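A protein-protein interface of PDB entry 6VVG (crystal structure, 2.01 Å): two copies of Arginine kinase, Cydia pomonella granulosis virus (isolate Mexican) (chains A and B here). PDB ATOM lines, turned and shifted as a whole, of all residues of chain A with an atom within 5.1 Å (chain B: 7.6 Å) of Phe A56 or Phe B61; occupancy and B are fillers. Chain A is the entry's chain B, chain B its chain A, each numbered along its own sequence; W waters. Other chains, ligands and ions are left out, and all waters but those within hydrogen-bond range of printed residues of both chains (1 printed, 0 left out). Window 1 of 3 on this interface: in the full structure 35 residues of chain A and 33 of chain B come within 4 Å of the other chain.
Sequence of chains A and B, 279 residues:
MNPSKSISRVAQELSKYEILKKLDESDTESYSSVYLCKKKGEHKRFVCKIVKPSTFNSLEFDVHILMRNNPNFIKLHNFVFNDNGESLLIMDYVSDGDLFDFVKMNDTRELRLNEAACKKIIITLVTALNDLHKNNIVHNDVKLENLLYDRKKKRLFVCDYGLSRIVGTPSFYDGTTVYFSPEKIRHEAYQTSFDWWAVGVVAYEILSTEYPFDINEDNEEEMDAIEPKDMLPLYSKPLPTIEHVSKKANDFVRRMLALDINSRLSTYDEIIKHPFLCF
Phe A56 touches Phe B61, and with the chains exchanged Phe A61 touches Phe B56.
Ser A58 touches Phe B61, and with the chains exchanged Phe A61 touches Ser B58.
Phe A61 touches Phe B79, and with the chains exchanged Phe A79 touches Phe B61.
Phe A79 touches its own counterpart, Phe B79.
Water W1 lies within hydrogen-bond range of the side-chain amide oxygen of Asn B78 and the backbone carbonyl oxygen of Phe A81.
Phe A56 touches one residue of chain B.
Phe B61 touches just these residues of chain A: Phe A56, Ser A58, Phe A79 and Phe A81.
Of the printed residues of chain B, Phe A61 touches Phe B56, Ser B58 and Phe B79.
Of the printed residues of chain A, Ser B58 touches Phe A61.
Printed residues of chain A within 4 Å of Val B80: Phe A79 (3.3 Å).
Of the printed residues of chain B, Phe A81 touches Phe B61 (3.6 Å), Ile B65 (3.4 Å), Leu B76 (3.8 Å), Asn B78 (3.4 Å) and Phe B79 (2.7 Å).
Printed residues of chain A within 4 Å of Leu B76: Phe A81.
His B64 touches none of the printed residues of chain A.
The nearest residue of chain A that does not touch Phe B61 is Phe A61 (4.1 Å).
Hydrophobic or aromatic side chains of chain B that line the printed part of chain A: Phe B56, Phe B61, Ile B65 and Phe B79.
Of the 13 printed residues of chain A, 5 touch a printed residue of chain B.
Among the printed residues, 15 pairs touch across the chains.
Among the printed residues, no Asp or Glu carboxylate lies within 4 Å of a Lys or Arg side-chain nitrogen of the other chain.
N of Phe A81 sits at hydrogen-bond distance from O of Phe B79 (2.7 Å).
Among the printed residues, merely in contact across the chains: Ser A58 with Ile B65 (3.2 Å), Phe A79 with Val B80 (3.3 Å), Phe A81 with Asn B78 (3.4 Å), Phe A81 with Ile B65 (3.4 Å), Ser A58 with Asp B62 (3.4 Å), Phe A79 with Phe B79 (3.5 Å), Phe A61 with Ser B58 (3.6 Å), Phe A79 with Phe B61 (3.6 Å), Phe A56 with Phe B61 (3.6 Å), Ser A58 with Phe B61 (3.6 Å), Phe A81 with Phe B61 (3.6 Å), Phe A81 with Leu B76 (3.8 Å), Phe A61 with Phe B56 (3.8 Å) and Phe A61 with Phe B79 (3.9 Å).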
ATOM      1  N   VAL A  51      -9.639  -5.307  11.519  1.00  0.00           N
ATOM      2  CA  VAL A  51      -8.278  -4.808  11.364  1.00  0.00           C
ATOM      3  C   VAL A  51      -7.815  -5.046   9.932  1.00  0.00           C
ATOM      4  O   VAL A  51      -8.143  -6.068   9.320  1.00  0.00           O
ATOM      5  CB  VAL A  51      -7.304  -5.462  12.361  1.00  0.00           C
ATOM      6  CG1 VAL A  51      -7.754  -5.210  13.799  1.00  0.00           C
ATOM      7  CG2 VAL A  51      -7.176  -6.960  12.091  1.00  0.00           C
ATOM      8  N   LYS A  52      -6.998  -4.123   9.429  1.00  0.00           N
ATOM      9  CA  LYS A  52      -6.605  -4.162   8.032  1.00  0.00           C
ATOM     10  C   LYS A  52      -5.731  -5.379   7.758  1.00  0.00           C
ATOM     11  O   LYS A  52      -4.867  -5.727   8.574  1.00  0.00           O
ATOM     12  CB  LYS A  52      -5.851  -2.895   7.640  1.00  0.00           C
ATOM     13  N   SER A  54      -2.658  -7.494   6.671  1.00  0.00           N
ATOM     14  CA  SER A  54      -1.210  -7.339   6.659  1.00  0.00           C
ATOM     15  C   SER A  54      -0.635  -6.491   7.789  1.00  0.00           C
ATOM     16  O   SER A  54       0.584  -6.462   7.936  1.00  0.00           O
ATOM     17  CB  SER A  54      -0.690  -6.727   5.344  1.00  0.00           C
ATOM     18  OG  SER A  54      -0.597  -5.308   5.493  1.00  0.00           O
ATOM     19  N   THR A  55      -1.444  -5.849   8.625  1.00  0.00           N
ATOM     20  CA  THR A  55      -0.908  -4.868   9.564  1.00  0.00           C
ATOM     21  C   THR A  55      -1.356  -5.139  10.995  1.00  0.00           C
ATOM     22  O   THR A  55      -1.315  -4.234  11.835  1.00  0.00           O
ATOM     23  CB  THR A  55      -1.305  -3.451   9.142  1.00  0.00           C
ATOM     24  OG1 THR A  55      -2.717  -3.275   9.316  1.00  0.00           O
ATOM     25  CG2 THR A  55      -0.943  -3.192   7.682  1.00  0.00           C
ATOM     26  N   PHE A  56      -1.767  -6.369  11.288  1.00  0.00           N
ATOM     27  CA  PHE A  56      -2.224  -6.738  12.621  1.00  0.00           C
ATOM     28  C   PHE A  56      -1.033  -7.122  13.491  1.00  0.00           C
ATOM     29  O   PHE A  56      -0.223  -7.973  13.111  1.00  0.00           O
ATOM     30  CB  PHE A  56      -3.223  -7.893  12.514  1.00  0.00           C
ATOM     31  CG  PHE A  56      -3.712  -8.415  13.834  1.00  0.00           C
ATOM     32  CD1 PHE A  56      -4.501  -7.633  14.658  1.00  0.00           C
ATOM     33  CD2 PHE A  56      -3.394  -9.702  14.243  1.00  0.00           C
ATOM     34  CE1 PHE A  56      -4.958  -8.117  15.870  1.00  0.00           C
ATOM     35  CE2 PHE A  56      -3.846 -10.192  15.456  1.00  0.00           C
ATOM     36  CZ  PHE A  56      -4.630  -9.400  16.269  1.00  0.00           C
ATOM     37  N   ASN A  57      -0.916  -6.472  14.648  1.00  0.00           N
ATOM     38  CA  ASN A  57       0.065  -6.855  15.658  1.00  0.00           C
ATOM     39  C   ASN A  57      -0.466  -8.088  16.379  1.00  0.00           C
ATOM     40  O   ASN A  57      -1.451  -8.005  17.119  1.00  0.00           O
ATOM     41  CB  ASN A  57       0.314  -5.704  16.630  1.00  0.00           C
ATOM     42  CG  ASN A  57       1.230  -6.091  17.783  1.00  0.00           C
ATOM     43  OD1 ASN A  57       1.744  -7.210  17.846  1.00  0.00           O
ATOM     44  ND2 ASN A  57       1.443  -5.156  18.700  1.00  0.00           N
ATOM     45  N   SER A  58       0.179  -9.235  16.158  1.00  0.00           N
ATOM     46  CA  SER A  58      -0.316 -10.483  16.728  1.00  0.00           C
ATOM     47  C   SER A  58      -0.472 -10.396  18.240  1.00  0.00           C
ATOM     48  O   SER A  58      -1.382 -11.010  18.807  1.00  0.00           O
ATOM     49  CB  SER A  58       0.628 -11.633  16.371  1.00  0.00           C
ATOM     50  OG  SER A  58       0.579 -11.926  14.987  1.00  0.00           O
ATOM     51  N   GLU A  60      -1.615  -8.155  20.061  1.00  0.00           N
ATOM     52  CA  GLU A  60      -2.906  -7.623  20.490  1.00  0.00           C
ATOM     53  C   GLU A  60      -3.835  -8.752  20.919  1.00  0.00           C
ATOM     54  O   GLU A  60      -4.551  -8.637  21.922  1.00  0.00           O
ATOM     55  CB  GLU A  60      -3.543  -6.805  19.367  1.00  0.00           C
ATOM     56  CG  GLU A  60      -4.909  -6.238  19.728  1.00  0.00           C
ATOM     57  CD  GLU A  60      -5.446  -5.267  18.692  1.00  0.00           C
ATOM     58  OE1 GLU A  60      -4.762  -5.034  17.672  1.00  0.00           O
ATOM     59  OE2 GLU A  60      -6.557  -4.737  18.899  1.00  0.00           O
ATOM     60  N   PHE A  61      -3.833  -9.854  20.168  1.00  0.00           N
ATOM     61  CA  PHE A  61      -4.613 -11.028  20.542  1.00  0.00           C
ATOM     62  C   PHE A  61      -4.148 -11.589  21.881  1.00  0.00           C
ATOM     63  O   PHE A  61      -4.970 -11.913  22.747  1.00  0.00           O
ATOM     64  CB  PHE A  61      -4.502 -12.067  19.422  1.00  0.00           C
ATOM     65  CG  PHE A  61      -5.118 -13.390  19.745  1.00  0.00           C
ATOM     66  CD1 PHE A  61      -6.486 -13.513  19.905  1.00  0.00           C
ATOM     67  CD2 PHE A  61      -4.326 -14.518  19.869  1.00  0.00           C
ATOM     68  CE1 PHE A  61      -7.053 -14.736  20.199  1.00  0.00           C
ATOM     69  CE2 PHE A  61      -4.886 -15.744  20.161  1.00  0.00           C
ATOM     70  CZ  PHE A  61      -6.250 -15.854  20.327  1.00  0.00           C
ATOM     71  N   PHE A  79     -12.050 -14.383  17.642  1.00  0.00           N
ATOM     72  CA  PHE A  79     -11.008 -13.788  16.818  1.00  0.00           C
ATOM     73  C   PHE A  79     -10.907 -14.616  15.547  1.00  0.00           C
ATOM     74  O   PHE A  79     -10.767 -15.841  15.615  1.00  0.00           O
ATOM     75  CB  PHE A  79      -9.664 -13.745  17.555  1.00  0.00           C
ATOM     76  CG  PHE A  79      -8.508 -13.317  16.693  1.00  0.00           C
ATOM     77  CD1 PHE A  79      -8.554 -12.132  15.971  1.00  0.00           C
ATOM     78  CD2 PHE A  79      -7.370 -14.099  16.611  1.00  0.00           C
ATOM     79  CE1 PHE A  79      -7.485 -11.744  15.180  1.00  0.00           C
ATOM     80  CE2 PHE A  79      -6.301 -13.718  15.826  1.00  0.00           C
ATOM     81  CZ  PHE A  79      -6.356 -12.541  15.110  1.00  0.00           C
ATOM     82  N   PHE A  81      -8.791 -14.808  11.936  1.00  0.00           N
ATOM     83  CA  PHE A  81      -7.656 -14.361  11.144  1.00  0.00           C
ATOM     84  C   PHE A  81      -7.715 -14.994   9.761  1.00  0.00           C
ATOM     85  O   PHE A  81      -7.992 -16.191   9.625  1.00  0.00           O
ATOM     86  CB  PHE A  81      -6.324 -14.714  11.813  1.00  0.00           C
ATOM     87  CG  PHE A  81      -5.127 -14.470  10.931  1.00  0.00           C
ATOM     88  CD1 PHE A  81      -4.537 -13.219  10.870  1.00  0.00           C
ATOM     89  CD2 PHE A  81      -4.598 -15.491  10.161  1.00  0.00           C
ATOM     90  CE1 PHE A  81      -3.441 -12.992  10.057  1.00  0.00           C
ATOM     91  CE2 PHE A  81      -3.504 -15.269   9.349  1.00  0.00           C
ATOM     92  CZ  PHE A  81      -2.926 -14.018   9.296  1.00  0.00           C
ATOM     93  N   SER A  87      -9.223  -9.452   9.207  1.00  0.00           N
ATOM     94  CA  SER A  87      -9.255 -10.111  10.500  1.00  0.00           C
ATOM     95  C   SER A  87     -10.258  -9.411  11.393  1.00  0.00           C
ATOM     96  O   SER A  87     -10.480  -8.204  11.270  1.00  0.00           O
ATOM     97  CB  SER A  87      -7.876 -10.080  11.148  1.00  0.00           C
ATOM     98  OG  SER A  87      -7.932 -10.021  12.561  1.00  0.00           O
ATOM     99  N   LEU A  89     -11.936  -9.023  15.523  1.00  0.00           N
ATOM    100  CA  LEU A  89     -11.934  -9.223  16.967  1.00  0.00           C
ATOM    101  C   LEU A  89     -13.301  -8.837  17.517  1.00  0.00           C
ATOM    102  O   LEU A  89     -13.768  -7.720  17.278  1.00  0.00           O
ATOM    103  CB  LEU A  89     -10.849  -8.387  17.648  1.00  0.00           C
ATOM    104  CG  LEU A  89      -9.393  -8.789  17.421  1.00  0.00           C
ATOM    105  CD1 LEU A  89      -8.968  -8.445  16.004  1.00  0.00           C
ATOM    106  CD2 LEU A  89      -8.490  -8.107  18.443  1.00  0.00           C
ATOM    107  N   PHE B  56      -6.168 -22.900  24.874  1.00  0.00           N
ATOM    108  CA  PHE B  56      -5.317 -22.359  23.824  1.00  0.00           C
ATOM    109  C   PHE B  56      -4.188 -21.515  24.405  1.00  0.00           C
ATOM    110  O   PHE B  56      -4.408 -20.684  25.290  1.00  0.00           O
ATOM    111  CB  PHE B  56      -6.134 -21.516  22.851  1.00  0.00           C
ATOM    112  CG  PHE B  56      -5.397 -21.169  21.592  1.00  0.00           C
ATOM    113  CD1 PHE B  56      -4.989 -22.166  20.726  1.00  0.00           C
ATOM    114  CD2 PHE B  56      -5.102 -19.852  21.279  1.00  0.00           C
ATOM    115  CE1 PHE B  56      -4.307 -21.861  19.568  1.00  0.00           C
ATOM    116  CE2 PHE B  56      -4.417 -19.540  20.117  1.00  0.00           C
ATOM    117  CZ  PHE B  56      -4.021 -20.548  19.262  1.00  0.00           C
ATOM    118  N   ASN B  57      -2.978 -21.734  23.891  1.00  0.00           N
ATOM    119  CA  ASN B  57      -1.829 -20.872  24.151  1.00  0.00           C
ATOM    120  C   ASN B  57      -1.796 -19.813  23.053  1.00  0.00           C
ATOM    121  O   ASN B  57      -1.456 -20.112  21.904  1.00  0.00           O
ATOM    122  CB  ASN B  57      -0.541 -21.693  24.180  1.00  0.00           C
ATOM    123  CG  ASN B  57       0.706 -20.835  24.306  1.00  0.00           C
ATOM    124  OD1 ASN B  57       0.633 -19.610  24.382  1.00  0.00           O
ATOM    125  ND2 ASN B  57       1.863 -21.483  24.331  1.00  0.00           N
ATOM    126  N   SER B  58      -2.151 -18.573  23.405  1.00  0.00           N
ATOM    127  CA  SER B  58      -2.294 -17.533  22.391  1.00  0.00           C
ATOM    128  C   SER B  58      -0.998 -17.299  21.626  1.00  0.00           C
ATOM    129  O   SER B  58      -1.032 -16.861  20.469  1.00  0.00           O
ATOM    130  CB  SER B  58      -2.771 -16.232  23.038  1.00  0.00           C
ATOM    131  OG  SER B  58      -1.782 -15.684  23.894  1.00  0.00           O
ATOM    132  N   LEU B  59       0.150 -17.581  22.243  1.00  0.00           N
ATOM    133  CA  LEU B  59       1.422 -17.370  21.563  1.00  0.00           C
ATOM    134  C   LEU B  59       1.586 -18.270  20.344  1.00  0.00           C
ATOM    135  O   LEU B  59       2.397 -17.961  19.464  1.00  0.00           O
ATOM    136  CB  LEU B  59       2.579 -17.605  22.531  1.00  0.00           C
ATOM    137  CG  LEU B  59       3.869 -16.827  22.264  1.00  0.00           C
ATOM    138  CD1 LEU B  59       3.638 -15.342  22.481  1.00  0.00           C
ATOM    139  CD2 LEU B  59       5.003 -17.337  23.143  1.00  0.00           C
ATOM    140  N   GLU B  60       0.845 -19.378  20.276  1.00  0.00           N
ATOM    141  CA  GLU B  60       0.909 -20.235  19.097  1.00  0.00           C
ATOM    142  C   GLU B  60       0.545 -19.457  17.840  1.00  0.00           C
ATOM    143  O   GLU B  60       1.140 -19.664  16.777  1.00  0.00           O
ATOM    144  CB  GLU B  60      -0.016 -21.439  19.273  1.00  0.00           C
ATOM    145  CG  GLU B  60       0.042 -22.439  18.131  1.00  0.00           C
ATOM    146  CD  GLU B  60      -0.668 -23.743  18.449  1.00  0.00           C
ATOM    147  OE1 GLU B  60      -1.304 -23.837  19.522  1.00  0.00           O
ATOM    148  OE2 GLU B  60      -0.591 -24.674  17.618  1.00  0.00           O
ATOM    149  N   PHE B  61      -0.421 -18.545  17.948  1.00  0.00           N
ATOM    150  CA  PHE B  61      -0.779 -17.699  16.812  1.00  0.00           C
ATOM    151  C   PHE B  61       0.393 -16.816  16.403  1.00  0.00           C
ATOM    152  O   PHE B  61       0.714 -16.698  15.215  1.00  0.00           O
ATOM    153  CB  PHE B  61      -2.007 -16.855  17.170  1.00  0.00           C
ATOM    154  CG  PHE B  61      -2.398 -15.864  16.110  1.00  0.00           C
ATOM    155  CD1 PHE B  61      -2.904 -16.292  14.894  1.00  0.00           C
ATOM    156  CD2 PHE B  61      -2.262 -14.504  16.334  1.00  0.00           C
ATOM    157  CE1 PHE B  61      -3.264 -15.383  13.917  1.00  0.00           C
ATOM    158  CE2 PHE B  61      -2.619 -13.590  15.360  1.00  0.00           C
ATOM    159  CZ  PHE B  61      -3.119 -14.031  14.149  1.00  0.00           C
ATOM    160  N   ASP B  62       1.058 -16.196  17.382  1.00  0.00           N
ATOM    161  CA  ASP B  62       2.146 -15.274  17.069  1.00  0.00           C
ATOM    162  C   ASP B  62       3.266 -15.967  16.305  1.00  0.00           C
ATOM    163  O   ASP B  62       3.828 -15.398  15.361  1.00  0.00           O
ATOM    164  CB  ASP B  62       2.702 -14.655  18.351  1.00  0.00           C
ATOM    165  CG  ASP B  62       1.644 -13.940  19.162  1.00  0.00           C
ATOM    166  OD1 ASP B  62       0.672 -14.600  19.575  1.00  0.00           O
ATOM    167  OD2 ASP B  62       1.786 -12.718  19.385  1.00  0.00           O
ATOM    168  N   VAL B  63       3.628 -17.185  16.714  1.00  0.00           N
ATOM    169  CA  VAL B  63       4.750 -17.868  16.080  1.00  0.00           C
ATOM    170  C   VAL B  63       4.476 -18.061  14.593  1.00  0.00           C
ATOM    171  O   VAL B  63       5.339 -17.804  13.747  1.00  0.00           O
ATOM    172  CB  VAL B  63       5.040 -19.206  16.783  1.00  0.00           C
ATOM    173  CG1 VAL B  63       6.104 -19.978  16.014  1.00  0.00           C
ATOM    174  CG2 VAL B  63       5.481 -18.958  18.219  1.00  0.00           C
ATOM    175  N   HIS B  64       3.268 -18.519  14.253  1.00  0.00           N
ATOM    176  CA  HIS B  64       2.908 -18.652  12.844  1.00  0.00           C
ATOM    177  C   HIS B  64       3.088 -17.328  12.116  1.00  0.00           C
ATOM    178  O   HIS B  64       3.740 -17.262  11.066  1.00  0.00           O
ATOM    179  CB  HIS B  64       1.461 -19.128  12.701  1.00  0.00           C
ATOM    180  CG  HIS B  64       1.236 -20.548  13.113  1.00  0.00           C
ATOM    181  ND1 HIS B  64       1.499 -21.616  12.284  1.00  0.00           N
ATOM    182  CD2 HIS B  64       0.752 -21.074  14.263  1.00  0.00           C
ATOM    183  CE1 HIS B  64       1.197 -22.740  12.910  1.00  0.00           C
ATOM    184  NE2 HIS B  64       0.743 -22.438  14.112  1.00  0.00           N
ATOM    185  N   ILE B  65       2.510 -16.257  12.665  1.00  0.00           N
ATOM    186  CA  ILE B  65       2.541 -14.960  11.998  1.00  0.00           C
ATOM    187  C   ILE B  65       3.968 -14.432  11.927  1.00  0.00           C
ATOM    188  O   ILE B  65       4.453 -14.043  10.857  1.00  0.00           O
ATOM    189  CB  ILE B  65       1.619 -13.960  12.721  1.00  0.00           C
ATOM    190  CG1 ILE B  65       0.172 -14.452  12.717  1.00  0.00           C
ATOM    191  CG2 ILE B  65       1.737 -12.579  12.084  1.00  0.00           C
ATOM    192  CD1 ILE B  65      -0.366 -14.798  11.353  1.00  0.00           C
ATOM    193  N   LEU B  66       4.655 -14.393  13.070  1.00  0.00           N
ATOM    194  CA  LEU B  66       5.997 -13.827  13.101  1.00  0.00           C
ATOM    195  C   LEU B  66       6.917 -14.532  12.114  1.00  0.00           C
ATOM    196  O   LEU B  66       7.773 -13.894  11.490  1.00  0.00           O
ATOM    197  CB  LEU B  66       6.567 -13.916  14.515  1.00  0.00           C
ATOM    198  CG  LEU B  66       5.982 -12.957  15.550  1.00  0.00           C
ATOM    199  CD1 LEU B  66       6.526 -13.277  16.941  1.00  0.00           C
ATOM    200  CD2 LEU B  66       6.277 -11.517  15.171  1.00  0.00           C
ATOM    201  N   MET B  67       6.754 -15.846  11.951  1.00  0.00           N
ATOM    202  CA  MET B  67       7.623 -16.641  11.095  1.00  0.00           C
ATOM    203  C   MET B  67       6.998 -16.927   9.734  1.00  0.00           C
ATOM    204  O   MET B  67       7.413 -17.871   9.051  1.00  0.00           O
ATOM    205  CB  MET B  67       7.982 -17.951  11.797  1.00  0.00           C
ATOM    206  CG  MET B  67       8.450 -17.782  13.237  1.00  0.00           C
ATOM    207  SD  MET B  67       9.708 -16.503  13.422  1.00  0.00           S
ATOM    208  CE  MET B  67      11.010 -17.158  12.379  1.00  0.00           C
ATOM    209  N   LEU B  76       0.216 -20.128   8.487  1.00  0.00           N
ATOM    210  CA  LEU B  76      -1.151 -20.198   8.990  1.00  0.00           C
ATOM    211  C   LEU B  76      -2.074 -19.473   8.018  1.00  0.00           C
ATOM    212  O   LEU B  76      -1.898 -18.278   7.764  1.00  0.00           O
ATOM    213  CB  LEU B  76      -1.254 -19.577  10.382  1.00  0.00           C
ATOM    214  CG  LEU B  76      -2.638 -19.622  11.029  1.00  0.00           C
ATOM    215  CD1 LEU B  76      -2.960 -21.043  11.468  1.00  0.00           C
ATOM    216  CD2 LEU B  76      -2.725 -18.659  12.203  1.00  0.00           C
ATOM    217  N   ASN B  78      -5.840 -19.780   8.048  1.00  0.00           N
ATOM    218  CA  ASN B  78      -7.013 -19.294   8.757  1.00  0.00           C
ATOM    219  C   ASN B  78      -6.904 -19.685  10.222  1.00  0.00           C
ATOM    220  O   ASN B  78      -6.234 -20.660  10.566  1.00  0.00           O
ATOM    221  CB  ASN B  78      -8.309 -19.857   8.167  1.00  0.00           C
ATOM    222  CG  ASN B  78      -8.441 -19.584   6.685  1.00  0.00           C
ATOM    223  OD1 ASN B  78      -9.068 -18.607   6.276  1.00  0.00           O
ATOM    224  ND2 ASN B  78      -7.845 -20.446   5.869  1.00  0.00           N
ATOM    225  N   PHE B  79      -7.576 -18.919  11.079  1.00  0.00           N
ATOM    226  CA  PHE B  79      -7.564 -19.175  12.512  1.00  0.00           C
ATOM    227  C   PHE B  79      -8.813 -18.545  13.107  1.00  0.00           C
ATOM    228  O   PHE B  79      -9.075 -17.357  12.894  1.00  0.00           O
ATOM    229  CB  PHE B  79      -6.290 -18.618  13.160  1.00  0.00           C
ATOM    230  CG  PHE B  79      -6.318 -18.615  14.659  1.00  0.00           C
ATOM    231  CD1 PHE B  79      -6.568 -19.778  15.376  1.00  0.00           C
ATOM    232  CD2 PHE B  79      -6.083 -17.443  15.354  1.00  0.00           C
ATOM    233  CE1 PHE B  79      -6.589 -19.758  16.763  1.00  0.00           C
ATOM    234  CE2 PHE B  79      -6.100 -17.418  16.731  1.00  0.00           C
ATOM    235  CZ  PHE B  79      -6.354 -18.573  17.439  1.00  0.00           C
ATOM    236  N   VAL B  80      -9.587 -19.351  13.823  1.00  0.00           N
ATOM    237  CA  VAL B  80     -10.808 -18.911  14.481  1.00  0.00           C
ATOM    238  C   VAL B  80     -10.693 -19.314  15.943  1.00  0.00           C
ATOM    239  O   VAL B  80     -10.656 -20.509  16.257  1.00  0.00           O
ATOM    240  CB  VAL B  80     -12.064 -19.520  13.846  1.00  0.00           C
ATOM    241  CG1 VAL B  80     -13.296 -19.029  14.585  1.00  0.00           C
ATOM    242  CG2 VAL B  80     -12.134 -19.181  12.369  1.00  0.00           C
ATOM    243  N   LEU B  89      -7.157 -23.901  13.650  1.00  0.00           N
ATOM    244  CA  LEU B  89      -5.999 -23.415  12.912  1.00  0.00           C
ATOM    245  C   LEU B  89      -5.900 -24.206  11.615  1.00  0.00           C
ATOM    246  O   LEU B  89      -5.731 -25.429  11.648  1.00  0.00           O
ATOM    247  CB  LEU B  89      -4.710 -23.561  13.720  1.00  0.00           C
ATOM    248  CG  LEU B  89      -4.463 -22.646  14.916  1.00  0.00           C
ATOM    249  CD1 LEU B  89      -5.342 -23.060  16.074  1.00  0.00           C
ATOM    250  CD2 LEU B  89      -2.990 -22.691  15.303  1.00  0.00           C
ATOM    251  N   TYR B 161       3.708 -24.969  17.685  1.00  0.00           N
ATOM    252  CA  TYR B 161       4.040 -23.830  18.532  1.00  0.00           C
ATOM    253  C   TYR B 161       3.103 -23.685  19.736  1.00  0.00           C
ATOM    254  O   TYR B 161       3.041 -22.605  20.335  1.00  0.00           O
ATOM    255  CB  TYR B 161       4.038 -22.558  17.682  1.00  0.00           C
ATOM    256  CG  TYR B 161       4.552 -22.800  16.269  1.00  0.00           C
ATOM    257  CD1 TYR B 161       5.682 -23.579  16.045  1.00  0.00           C
ATOM    258  CD2 TYR B 161       3.902 -22.263  15.165  1.00  0.00           C
ATOM    259  CE1 TYR B 161       6.150 -23.813  14.766  1.00  0.00           C
ATOM    260  CE2 TYR B 161       4.367 -22.486  13.884  1.00  0.00           C
ATOM    261  CZ  TYR B 161       5.491 -23.265  13.691  1.00  0.00           C
ATOM    262  OH  TYR B 161       5.957 -23.497  12.419  1.00  0.00           O
ATOM    263  N   GLY B 162       2.416 -24.759  20.130  1.00  0.00           N
ATOM    264  CA  GLY B 162       1.426 -24.678  21.193  1.00  0.00           C
ATOM    265  C   GLY B 162       1.998 -24.522  22.587  1.00  0.00           C
ATOM    266  O   GLY B 162       1.261 -24.144  23.505  1.00  0.00           O
ATOM    267  N   SER B 164       4.868 -22.612  23.025  1.00  0.00           N
ATOM    268  CA  SER B 164       5.784 -21.486  22.911  1.00  0.00           C
ATOM    269  C   SER B 164       5.575 -20.497  24.054  1.00  0.00           C
ATOM    270  O   SER B 164       4.462 -20.327  24.562  1.00  0.00           O
ATOM    271  CB  SER B 164       5.586 -20.777  21.570  1.00  0.00           C
ATOM    272  OG  SER B 164       6.004 -21.595  20.488  1.00  0.00           O
HETATM  273  O   HOH W   1     -10.656 -17.731   8.783  1.00  0.00           O
